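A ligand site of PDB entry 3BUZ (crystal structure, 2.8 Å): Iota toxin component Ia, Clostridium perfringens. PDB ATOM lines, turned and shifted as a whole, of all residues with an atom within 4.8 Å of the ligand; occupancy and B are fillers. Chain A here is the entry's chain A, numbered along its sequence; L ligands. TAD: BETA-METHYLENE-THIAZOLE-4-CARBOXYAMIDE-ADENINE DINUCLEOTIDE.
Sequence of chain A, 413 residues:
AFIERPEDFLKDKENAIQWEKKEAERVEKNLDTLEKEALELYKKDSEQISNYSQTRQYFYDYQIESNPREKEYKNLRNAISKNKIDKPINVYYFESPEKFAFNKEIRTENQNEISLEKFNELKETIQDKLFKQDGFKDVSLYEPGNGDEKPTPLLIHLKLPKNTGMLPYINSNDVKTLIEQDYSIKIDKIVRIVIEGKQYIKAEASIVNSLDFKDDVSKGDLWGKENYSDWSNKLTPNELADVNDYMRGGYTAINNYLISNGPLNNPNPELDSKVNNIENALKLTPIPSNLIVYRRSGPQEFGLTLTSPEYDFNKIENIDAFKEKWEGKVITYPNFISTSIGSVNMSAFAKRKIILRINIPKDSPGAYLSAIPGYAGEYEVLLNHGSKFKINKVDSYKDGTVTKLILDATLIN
OE1 of Glu 380 lies within hydrogen-bond range of OG of Ser 338, 2.4 Å away.
OE1 of Glu 301 lies within salt-bridge range of NE of Arg 295 (2.7 Å).
OH of Tyr 333 sits at hydrogen-bond distance from OE1 of Glu 301, at 2.6 Å.
O of Arg 296 lies within hydrogen-bond range of NH1 of Arg 352, at 3.0 Å.
NH1 of Arg 295 is in hydrogen-bond range of O of Ser 338, at 3.2 Å.
N of Tyr 294 is in hydrogen-bond range of O of Ser 340, 2.7 Å away.
N of Gly 298 lies within hydrogen-bond range of OE2 of Glu 301 (2.8 Å).
OG of Ser 338 lies close to OH of Tyr 246.
An oxygen (O2D) of the ligand is in hydrogen-bond range of the side-chain hydroxyl (OG) of Ser 338.
OD1 of Asn 335 lies within hydrogen-bond range of N6A of the ligand (2.5 Å).
The backbone NH (N) of Arg 296 sits at hydrogen-bond distance from an oxygen (O6N) of the ligand (2.5 Å).
O2B of the ligand lies close to O of Gly 298.
N of Gly 298 sits close to O2B of the ligand (3.4 Å).
NH1 of Arg 352 lies within salt-bridge range of O1N of the ligand, 2.8 Å away.
An oxygen (O2B) of the ligand is in hydrogen-bond range of the side-chain carboxylate (OE2) of Glu 301 (3.1 Å).
The side-chain amide nitrogen (ND2) of Asn 255 lies within hydrogen-bond range of an oxygen (O2A) of the ligand (2.6 Å).
An oxygen (O2D) of the ligand is in hydrogen-bond range of the side-chain carboxylate (OE1) of Glu 380 (2.7 Å).
The backbone carbonyl oxygen (O) of Arg 296 sits at hydrogen-bond distance from a nitrogen (N6N) of the ligand (2.9 Å).
NH2 of Arg 295 is in salt-bridge range of O1A of the ligand, at 3.0 Å.
Residues that only touch the ligand: Gln 300, Tyr 251, Tyr 333, Phe 349, Pro 334, Ile 259, Ser 340 and Thr 339.
Hydrophobic or aromatic side chains that line the ligand: Tyr 251, Ile 259, Tyr 333, Pro 334 and Phe 349.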
ATOM      1  N   TYR A 246      -7.468  14.527 -15.805  1.00  0.00           N
ATOM      2  CA  TYR A 246      -6.156  13.910 -16.219  1.00  0.00           C
ATOM      3  C   TYR A 246      -6.414  12.400 -16.400  1.00  0.00           C
ATOM      4  O   TYR A 246      -5.863  11.731 -17.302  1.00  0.00           O
ATOM      5  CB  TYR A 246      -5.071  14.238 -15.146  1.00  0.00           C
ATOM      6  CG  TYR A 246      -3.577  13.834 -15.351  1.00  0.00           C
ATOM      7  CD1 TYR A 246      -3.186  12.507 -15.664  1.00  0.00           C
ATOM      8  CD2 TYR A 246      -2.548  14.761 -15.108  1.00  0.00           C
ATOM      9  CE1 TYR A 246      -1.809  12.137 -15.793  1.00  0.00           C
ATOM     10  CE2 TYR A 246      -1.163  14.394 -15.253  1.00  0.00           C
ATOM     11  CZ  TYR A 246      -0.808  13.096 -15.589  1.00  0.00           C
ATOM     12  OH  TYR A 246       0.531  12.749 -15.712  1.00  0.00           O
ATOM     13  N   TYR A 251      -3.760  13.004 -21.484  1.00  0.00           N
ATOM     14  CA  TYR A 251      -2.926  13.764 -20.564  1.00  0.00           C
ATOM     15  C   TYR A 251      -2.029  14.718 -21.368  1.00  0.00           C
ATOM     16  O   TYR A 251      -1.496  15.684 -20.819  1.00  0.00           O
ATOM     17  CB  TYR A 251      -2.043  12.781 -19.802  1.00  0.00           C
ATOM     18  CG  TYR A 251      -1.501  11.687 -20.716  1.00  0.00           C
ATOM     19  CD1 TYR A 251      -1.980  10.378 -20.650  1.00  0.00           C
ATOM     20  CD2 TYR A 251      -0.528  11.976 -21.685  1.00  0.00           C
ATOM     21  CE1 TYR A 251      -1.495   9.399 -21.504  1.00  0.00           C
ATOM     22  CE2 TYR A 251      -0.039  11.016 -22.528  1.00  0.00           C
ATOM     23  CZ  TYR A 251      -0.516   9.726 -22.451  1.00  0.00           C
ATOM     24  OH  TYR A 251       0.010   8.782 -23.313  1.00  0.00           O
ATOM     25  N   THR A 252      -1.838  14.419 -22.651  1.00  0.00           N
ATOM     26  CA  THR A 252      -1.020  15.270 -23.528  1.00  0.00           C
ATOM     27  C   THR A 252      -1.754  16.569 -23.910  1.00  0.00           C
ATOM     28  O   THR A 252      -1.297  17.314 -24.794  1.00  0.00           O
ATOM     29  CB  THR A 252      -0.440  14.519 -24.772  1.00  0.00           C
ATOM     30  OG1 THR A 252      -1.337  13.492 -25.199  1.00  0.00           O
ATOM     31  CG2 THR A 252       0.926  13.882 -24.456  1.00  0.00           C
ATOM     32  N   ASN A 255      -0.937  18.149 -19.459  1.00  0.00           N
ATOM     33  CA  ASN A 255       0.506  18.432 -19.337  1.00  0.00           C
ATOM     34  C   ASN A 255       0.946  19.489 -20.325  1.00  0.00           C
ATOM     35  O   ASN A 255       1.510  20.520 -19.924  1.00  0.00           O
ATOM     36  CB  ASN A 255       1.409  17.195 -19.509  1.00  0.00           C
ATOM     37  CG  ASN A 255       1.200  16.166 -18.445  1.00  0.00           C
ATOM     38  OD1 ASN A 255       0.812  16.481 -17.324  1.00  0.00           O
ATOM     39  ND2 ASN A 255       1.428  14.918 -18.810  1.00  0.00           N
ATOM     40  N   ILE A 259       3.501  22.580 -19.533  1.00  0.00           N
ATOM     41  CA  ILE A 259       4.853  22.608 -20.100  1.00  0.00           C
ATOM     42  C   ILE A 259       5.215  24.006 -20.625  1.00  0.00           C
ATOM     43  O   ILE A 259       5.821  24.810 -19.913  1.00  0.00           O
ATOM     44  CB  ILE A 259       5.002  21.565 -21.275  1.00  0.00           C
ATOM     45  CG1 ILE A 259       4.329  20.217 -20.970  1.00  0.00           C
ATOM     46  CG2 ILE A 259       6.476  21.411 -21.738  1.00  0.00           C
ATOM     47  CD1 ILE A 259       4.913  19.401 -19.848  1.00  0.00           C
ATOM     48  N   TYR A 294       8.489   5.235  -8.952  1.00  0.00           N
ATOM     49  CA  TYR A 294       9.341   5.133 -10.123  1.00  0.00           C
ATOM     50  C   TYR A 294       8.680   5.812 -11.259  1.00  0.00           C
ATOM     51  O   TYR A 294       7.530   5.528 -11.495  1.00  0.00           O
ATOM     52  CB  TYR A 294       9.657   3.674 -10.443  1.00  0.00           C
ATOM     53  CG  TYR A 294      10.432   2.960  -9.346  1.00  0.00           C
ATOM     54  CD1 TYR A 294       9.793   2.419  -8.275  1.00  0.00           C
ATOM     55  CD2 TYR A 294      11.799   2.809  -9.445  1.00  0.00           C
ATOM     56  CE1 TYR A 294      10.460   1.775  -7.309  1.00  0.00           C
ATOM     57  CE2 TYR A 294      12.505   2.142  -8.486  1.00  0.00           C
ATOM     58  CZ  TYR A 294      11.819   1.652  -7.401  1.00  0.00           C
ATOM     59  OH  TYR A 294      12.493   1.021  -6.397  1.00  0.00           O
ATOM     60  N   ARG A 295       9.393   6.739 -11.919  1.00  0.00           N
ATOM     61  CA  ARG A 295       8.923   7.364 -13.160  1.00  0.00           C
ATOM     62  C   ARG A 295       9.752   7.032 -14.371  1.00  0.00           C
ATOM     63  O   ARG A 295      10.970   7.137 -14.374  1.00  0.00           O
ATOM     64  CB  ARG A 295       8.865   8.862 -13.071  1.00  0.00           C
ATOM     65  CG  ARG A 295       8.384   9.391 -14.404  1.00  0.00           C
ATOM     66  CD  ARG A 295       8.204  10.865 -14.406  1.00  0.00           C
ATOM     67  NE  ARG A 295       8.069  11.309 -15.787  1.00  0.00           N
ATOM     68  CZ  ARG A 295       6.935  11.276 -16.495  1.00  0.00           C
ATOM     69  NH1 ARG A 295       5.787  10.811 -15.944  1.00  0.00           N
ATOM     70  NH2 ARG A 295       6.958  11.730 -17.760  1.00  0.00           N
ATOM     71  N   ARG A 296       9.110   6.636 -15.426  1.00  0.00           N
ATOM     72  CA  ARG A 296       9.955   6.294 -16.561  1.00  0.00           C
ATOM     73  C   ARG A 296       9.909   7.531 -17.399  1.00  0.00           C
ATOM     74  O   ARG A 296       8.823   8.046 -17.735  1.00  0.00           O
ATOM     75  CB  ARG A 296       9.459   5.025 -17.296  1.00  0.00           C
ATOM     76  CG  ARG A 296      10.120   3.712 -16.827  1.00  0.00           C
ATOM     77  CD  ARG A 296      10.529   2.895 -18.051  1.00  0.00           C
ATOM     78  NE  ARG A 296      11.294   1.661 -17.816  1.00  0.00           N
ATOM     79  CZ  ARG A 296      11.264   1.051 -16.666  1.00  0.00           C
ATOM     80  NH1 ARG A 296      10.508   1.607 -15.754  1.00  0.00           N
ATOM     81  NH2 ARG A 296      11.945  -0.057 -16.459  1.00  0.00           N
ATOM     82  N   SER A 297      11.034   8.123 -17.688  1.00  0.00           N
ATOM     83  CA  SER A 297      10.805   9.410 -18.335  1.00  0.00           C
ATOM     84  C   SER A 297      11.378   9.534 -19.774  1.00  0.00           C
ATOM     85  O   SER A 297      12.337   8.801 -20.155  1.00  0.00           O
ATOM     86  CB  SER A 297      11.243  10.536 -17.383  1.00  0.00           C
ATOM     87  OG  SER A 297      12.639  10.498 -17.308  1.00  0.00           O
ATOM     88  N   GLY A 298      10.832  10.433 -20.582  1.00  0.00           N
ATOM     89  CA  GLY A 298      11.333  10.521 -21.970  1.00  0.00           C
ATOM     90  C   GLY A 298      12.305  11.640 -22.205  1.00  0.00           C
ATOM     91  O   GLY A 298      12.406  12.508 -21.373  1.00  0.00           O
ATOM     92  N   PRO A 299      12.957  11.699 -23.364  1.00  0.00           N
ATOM     93  CA  PRO A 299      14.029  12.683 -23.643  1.00  0.00           C
ATOM     94  C   PRO A 299      13.669  14.165 -23.390  1.00  0.00           C
ATOM     95  O   PRO A 299      14.490  14.879 -22.863  1.00  0.00           O
ATOM     96  CB  PRO A 299      14.341  12.485 -25.129  1.00  0.00           C
ATOM     97  CG  PRO A 299      13.679  11.245 -25.542  1.00  0.00           C
ATOM     98  CD  PRO A 299      12.608  10.891 -24.545  1.00  0.00           C
ATOM     99  N   GLN A 300      12.469  14.625 -23.775  1.00  0.00           N
ATOM    100  CA  GLN A 300      12.091  16.015 -23.457  1.00  0.00           C
ATOM    101  C   GLN A 300      12.458  16.353 -22.009  1.00  0.00           C
ATOM    102  O   GLN A 300      13.300  17.237 -21.780  1.00  0.00           O
ATOM    103  CB  GLN A 300      10.590  16.260 -23.656  1.00  0.00           C
ATOM    104  CG  GLN A 300      10.205  16.778 -24.968  1.00  0.00           C
ATOM    105  CD  GLN A 300      10.486  15.781 -26.057  1.00  0.00           C
ATOM    106  OE1 GLN A 300      11.271  16.031 -26.995  1.00  0.00           O
ATOM    107  NE2 GLN A 300       9.847  14.616 -25.940  1.00  0.00           N
ATOM    108  N   GLU A 301      11.868  15.662 -21.033  1.00  0.00           N
ATOM    109  CA  GLU A 301      12.093  16.048 -19.633  1.00  0.00           C
ATOM    110  C   GLU A 301      13.576  16.324 -19.321  1.00  0.00           C
ATOM    111  O   GLU A 301      13.896  16.885 -18.301  1.00  0.00           O
ATOM    112  CB  GLU A 301      11.546  15.002 -18.665  1.00  0.00           C
ATOM    113  CG  GLU A 301      10.028  14.758 -18.711  1.00  0.00           C
ATOM    114  CD  GLU A 301       9.678  13.323 -18.323  1.00  0.00           C
ATOM    115  OE1 GLU A 301       9.662  13.077 -17.087  1.00  0.00           O
ATOM    116  OE2 GLU A 301       9.454  12.475 -19.250  1.00  0.00           O
ATOM    117  N   TYR A 333       9.236  20.499 -12.367  1.00  0.00           N
ATOM    118  CA  TYR A 333       8.281  19.922 -13.294  1.00  0.00           C
ATOM    119  C   TYR A 333       7.021  20.806 -13.370  1.00  0.00           C
ATOM    120  O   TYR A 333       6.273  20.978 -12.390  1.00  0.00           O
ATOM    121  CB  TYR A 333       7.952  18.447 -12.897  1.00  0.00           C
ATOM    122  CG  TYR A 333       8.821  17.362 -13.574  1.00  0.00           C
ATOM    123  CD1 TYR A 333       8.357  16.670 -14.683  1.00  0.00           C
ATOM    124  CD2 TYR A 333      10.094  17.030 -13.096  1.00  0.00           C
ATOM    125  CE1 TYR A 333       9.132  15.706 -15.284  1.00  0.00           C
ATOM    126  CE2 TYR A 333      10.869  16.052 -13.700  1.00  0.00           C
ATOM    127  CZ  TYR A 333      10.376  15.396 -14.801  1.00  0.00           C
ATOM    128  OH  TYR A 333      11.124  14.433 -15.434  1.00  0.00           O
ATOM    129  N   PRO A 334       6.790  21.416 -14.546  1.00  0.00           N
ATOM    130  CA  PRO A 334       5.523  22.132 -14.548  1.00  0.00           C
ATOM    131  C   PRO A 334       4.334  21.165 -14.485  1.00  0.00           C
ATOM    132  O   PRO A 334       3.350  21.489 -13.806  1.00  0.00           O
ATOM    133  CB  PRO A 334       5.573  22.927 -15.860  1.00  0.00           C
ATOM    134  CG  PRO A 334       7.039  22.819 -16.363  1.00  0.00           C
ATOM    135  CD  PRO A 334       7.520  21.517 -15.824  1.00  0.00           C
ATOM    136  N   ASN A 335       4.421  19.985 -15.130  1.00  0.00           N
ATOM    137  CA  ASN A 335       3.313  18.982 -15.159  1.00  0.00           C
ATOM    138  C   ASN A 335       3.015  18.228 -13.867  1.00  0.00           C
ATOM    139  O   ASN A 335       3.927  17.968 -13.074  1.00  0.00           O
ATOM    140  CB  ASN A 335       3.462  17.944 -16.289  1.00  0.00           C
ATOM    141  CG  ASN A 335       4.907  17.561 -16.582  1.00  0.00           C
ATOM    142  OD1 ASN A 335       5.828  18.346 -16.356  1.00  0.00           O
ATOM    143  ND2 ASN A 335       5.112  16.350 -17.149  1.00  0.00           N
ATOM    144  N   SER A 338       3.714  11.812 -13.004  1.00  0.00           N
ATOM    145  CA  SER A 338       2.898  10.620 -13.085  1.00  0.00           C
ATOM    146  C   SER A 338       3.732   9.412 -12.821  1.00  0.00           C
ATOM    147  O   SER A 338       4.366   8.921 -13.738  1.00  0.00           O
ATOM    148  CB  SER A 338       2.337  10.505 -14.502  1.00  0.00           C
ATOM    149  OG  SER A 338       1.229   9.649 -14.542  1.00  0.00           O
ATOM    150  N   THR A 339       3.737   8.903 -11.612  1.00  0.00           N
ATOM    151  CA  THR A 339       4.682   7.833 -11.318  1.00  0.00           C
ATOM    152  C   THR A 339       4.003   6.515 -10.946  1.00  0.00           C
ATOM    153  O   THR A 339       2.840   6.489 -10.544  1.00  0.00           O
ATOM    154  CB  THR A 339       5.521   8.220 -10.106  1.00  0.00           C
ATOM    155  OG1 THR A 339       4.696   8.192  -8.940  1.00  0.00           O
ATOM    156  CG2 THR A 339       6.045   9.624 -10.257  1.00  0.00           C
ATOM    157  N   SER A 340       4.751   5.444 -10.996  1.00  0.00           N
ATOM    158  CA  SER A 340       4.258   4.210 -10.525  1.00  0.00           C
ATOM    159  C   SER A 340       4.938   3.674  -9.220  1.00  0.00           C
ATOM    160  O   SER A 340       6.114   3.939  -9.001  1.00  0.00           O
ATOM    161  CB  SER A 340       4.424   3.215 -11.626  1.00  0.00           C
ATOM    162  OG  SER A 340       4.182   1.942 -11.077  1.00  0.00           O
ATOM    163  N   ALA A 348       3.280   0.802 -22.114  1.00  0.00           N
ATOM    164  CA  ALA A 348       3.148   2.258 -22.322  1.00  0.00           C
ATOM    165  C   ALA A 348       4.487   3.005 -22.481  1.00  0.00           C
ATOM    166  O   ALA A 348       4.538   3.981 -23.278  1.00  0.00           O
ATOM    167  CB  ALA A 348       2.328   2.892 -21.238  1.00  0.00           C
ATOM    168  N   PHE A 349       5.543   2.579 -21.770  1.00  0.00           N
ATOM    169  CA  PHE A 349       6.863   3.192 -21.910  1.00  0.00           C
ATOM    170  C   PHE A 349       8.049   2.216 -22.024  1.00  0.00           C
ATOM    171  O   PHE A 349       9.209   2.524 -21.600  1.00  0.00           O
ATOM    172  CB  PHE A 349       7.074   4.095 -20.761  1.00  0.00           C
ATOM    173  CG  PHE A 349       6.696   3.476 -19.466  1.00  0.00           C
ATOM    174  CD1 PHE A 349       7.580   2.630 -18.807  1.00  0.00           C
ATOM    175  CD2 PHE A 349       5.467   3.761 -18.877  1.00  0.00           C
ATOM    176  CE1 PHE A 349       7.234   2.056 -17.560  1.00  0.00           C
ATOM    177  CE2 PHE A 349       5.116   3.190 -17.607  1.00  0.00           C
ATOM    178  CZ  PHE A 349       5.983   2.336 -16.975  1.00  0.00           C
ATOM    179  N   ARG A 352      11.445   3.900 -23.116  1.00  0.00           N
ATOM    180  CA  ARG A 352      12.068   5.019 -22.397  1.00  0.00           C
ATOM    181  C   ARG A 352      13.285   4.617 -21.604  1.00  0.00           C
ATOM    182  O   ARG A 352      13.353   3.538 -21.009  1.00  0.00           O
ATOM    183  CB  ARG A 352      11.113   5.738 -21.472  1.00  0.00           C
ATOM    184  CG  ARG A 352      10.018   6.401 -22.195  1.00  0.00           C
ATOM    185  CD  ARG A 352       9.149   7.154 -21.252  1.00  0.00           C
ATOM    186  NE  ARG A 352       7.949   7.646 -21.925  1.00  0.00           N
ATOM    187  CZ  ARG A 352       7.049   8.438 -21.365  1.00  0.00           C
ATOM    188  NH1 ARG A 352       7.177   8.841 -20.088  1.00  0.00           N
ATOM    189  NH2 ARG A 352       5.966   8.789 -22.057  1.00  0.00           N
ATOM    190  N   GLU A 378      -2.373  -0.191 -13.238  1.00  0.00           N
ATOM    191  CA  GLU A 378      -0.951   0.220 -13.512  1.00  0.00           C
ATOM    192  C   GLU A 378      -0.235   0.887 -12.322  1.00  0.00           C
ATOM    193  O   GLU A 378       0.918   1.328 -12.421  1.00  0.00           O
ATOM    194  CB  GLU A 378      -0.782   1.010 -14.835  1.00  0.00           C
ATOM    195  CG  GLU A 378      -1.143   2.498 -14.780  1.00  0.00           C
ATOM    196  CD  GLU A 378      -2.650   2.757 -14.672  1.00  0.00           C
ATOM    197  OE1 GLU A 378      -3.278   2.350 -13.654  1.00  0.00           O
ATOM    198  OE2 GLU A 378      -3.225   3.393 -15.592  1.00  0.00           O
ATOM    199  N   GLU A 380      -0.519   3.575 -10.187  1.00  0.00           N
ATOM    200  CA  GLU A 380      -0.078   4.909 -10.432  1.00  0.00           C
ATOM    201  C   GLU A 380      -0.197   5.770  -9.193  1.00  0.00           C
ATOM    202  O   GLU A 380      -1.171   5.671  -8.433  1.00  0.00           O
ATOM    203  CB  GLU A 380      -0.858   5.492 -11.587  1.00  0.00           C
ATOM    204  CG  GLU A 380      -0.469   6.895 -11.939  1.00  0.00           C
ATOM    205  CD  GLU A 380      -1.184   7.439 -13.168  1.00  0.00           C
ATOM    206  OE1 GLU A 380      -0.762   8.552 -13.629  1.00  0.00           O
ATOM    207  OE2 GLU A 380      -2.146   6.769 -13.693  1.00  0.00           O
HETATM  208  PA  TAD L   1       3.768  12.696 -19.646  1.00  0.00           P
HETATM  209  O1A TAD L   1       4.548  13.422 -18.545  1.00  0.00           O
HETATM  210  O2A TAD L   1       2.640  13.308 -20.425  1.00  0.00           O
HETATM  211  O5B TAD L   1       4.854  12.336 -20.798  1.00  0.00           O
HETATM  212  C5B TAD L   1       4.524  12.574 -22.170  1.00  0.00           C
HETATM  213  C4B TAD L   1       5.648  13.037 -23.117  1.00  0.00           C
HETATM  214  O4B TAD L   1       6.004  14.428 -22.953  1.00  0.00           O
HETATM  215  C3B TAD L   1       6.924  12.268 -22.973  1.00  0.00           C
HETATM  216  O3B TAD L   1       7.526  12.228 -24.263  1.00  0.00           O
HETATM  217  C2B TAD L   1       7.754  13.165 -22.081  1.00  0.00           C
HETATM  218  O2B TAD L   1       9.165  12.933 -22.260  1.00  0.00           O
HETATM  219  C1B TAD L   1       7.314  14.577 -22.434  1.00  0.00           C
HETATM  220  N9A TAD L   1       7.292  15.347 -21.169  1.00  0.00           N
HETATM  221  C8A TAD L   1       6.625  14.964 -20.049  1.00  0.00           C
HETATM  222  N7A TAD L   1       6.788  15.853 -19.026  1.00  0.00           N
HETATM  223  C5A TAD L   1       7.603  16.836 -19.502  1.00  0.00           C
HETATM  224  C6A TAD L   1       8.192  18.104 -18.957  1.00  0.00           C
HETATM  225  N6A TAD L   1       7.959  18.495 -17.689  1.00  0.00           N
HETATM  226  N1A TAD L   1       8.966  18.855 -19.795  1.00  0.00           N
HETATM  227  C2A TAD L   1       9.219  18.455 -21.063  1.00  0.00           C
HETATM  228  N3A TAD L   1       8.715  17.327 -21.609  1.00  0.00           N
HETATM  229  C4A TAD L   1       7.919  16.498 -20.910  1.00  0.00           C
HETATM  230  C3  TAD L   1       2.965  11.394 -18.659  1.00  0.00           C
HETATM  231  PN  TAD L   1       3.271   9.892 -19.593  1.00  0.00           P
HETATM  232  O1N TAD L   1       4.597   9.269 -19.227  1.00  0.00           O
HETATM  233  O2N TAD L   1       3.056  10.265 -21.054  1.00  0.00           O
HETATM  234  O5D TAD L   1       2.109   8.848 -19.205  1.00  0.00           O
HETATM  235  C5D TAD L   1       1.661   7.830 -20.116  1.00  0.00           C
HETATM  236  C4D TAD L   1       0.512   7.125 -19.455  1.00  0.00           C
HETATM  237  O4D TAD L   1       1.049   6.092 -18.631  1.00  0.00           O
HETATM  238  C3D TAD L   1      -0.269   8.059 -18.541  1.00  0.00           C
HETATM  239  O3D TAD L   1      -1.652   7.706 -18.618  1.00  0.00           O
HETATM  240  C2D TAD L   1       0.220   7.763 -17.142  1.00  0.00           C
HETATM  241  O2D TAD L   1      -0.900   7.836 -16.268  1.00  0.00           O
HETATM  242  C1D TAD L   1       0.831   6.362 -17.237  1.00  0.00           C
HETATM  243  C2N TAD L   1       2.129   6.222 -16.513  1.00  0.00           C
HETATM  244  N3N TAD L   1       3.399   6.565 -16.867  1.00  0.00           N
HETATM  245  C4N TAD L   1       4.330   6.252 -15.934  1.00  0.00           C
HETATM  246  C5N TAD L   1       3.781   5.631 -14.819  1.00  0.00           C
HETATM  247  S1N TAD L   1       2.039   5.430 -14.963  1.00  0.00           S
HETATM  248  C6N TAD L   1       5.768   6.564 -16.123  1.00  0.00           C
HETATM  249  O6N TAD L   1       6.644   6.081 -15.431  1.00  0.00           O
HETATM  250  N6N TAD L   1       6.056   7.424 -17.092  1.00  0.00           N
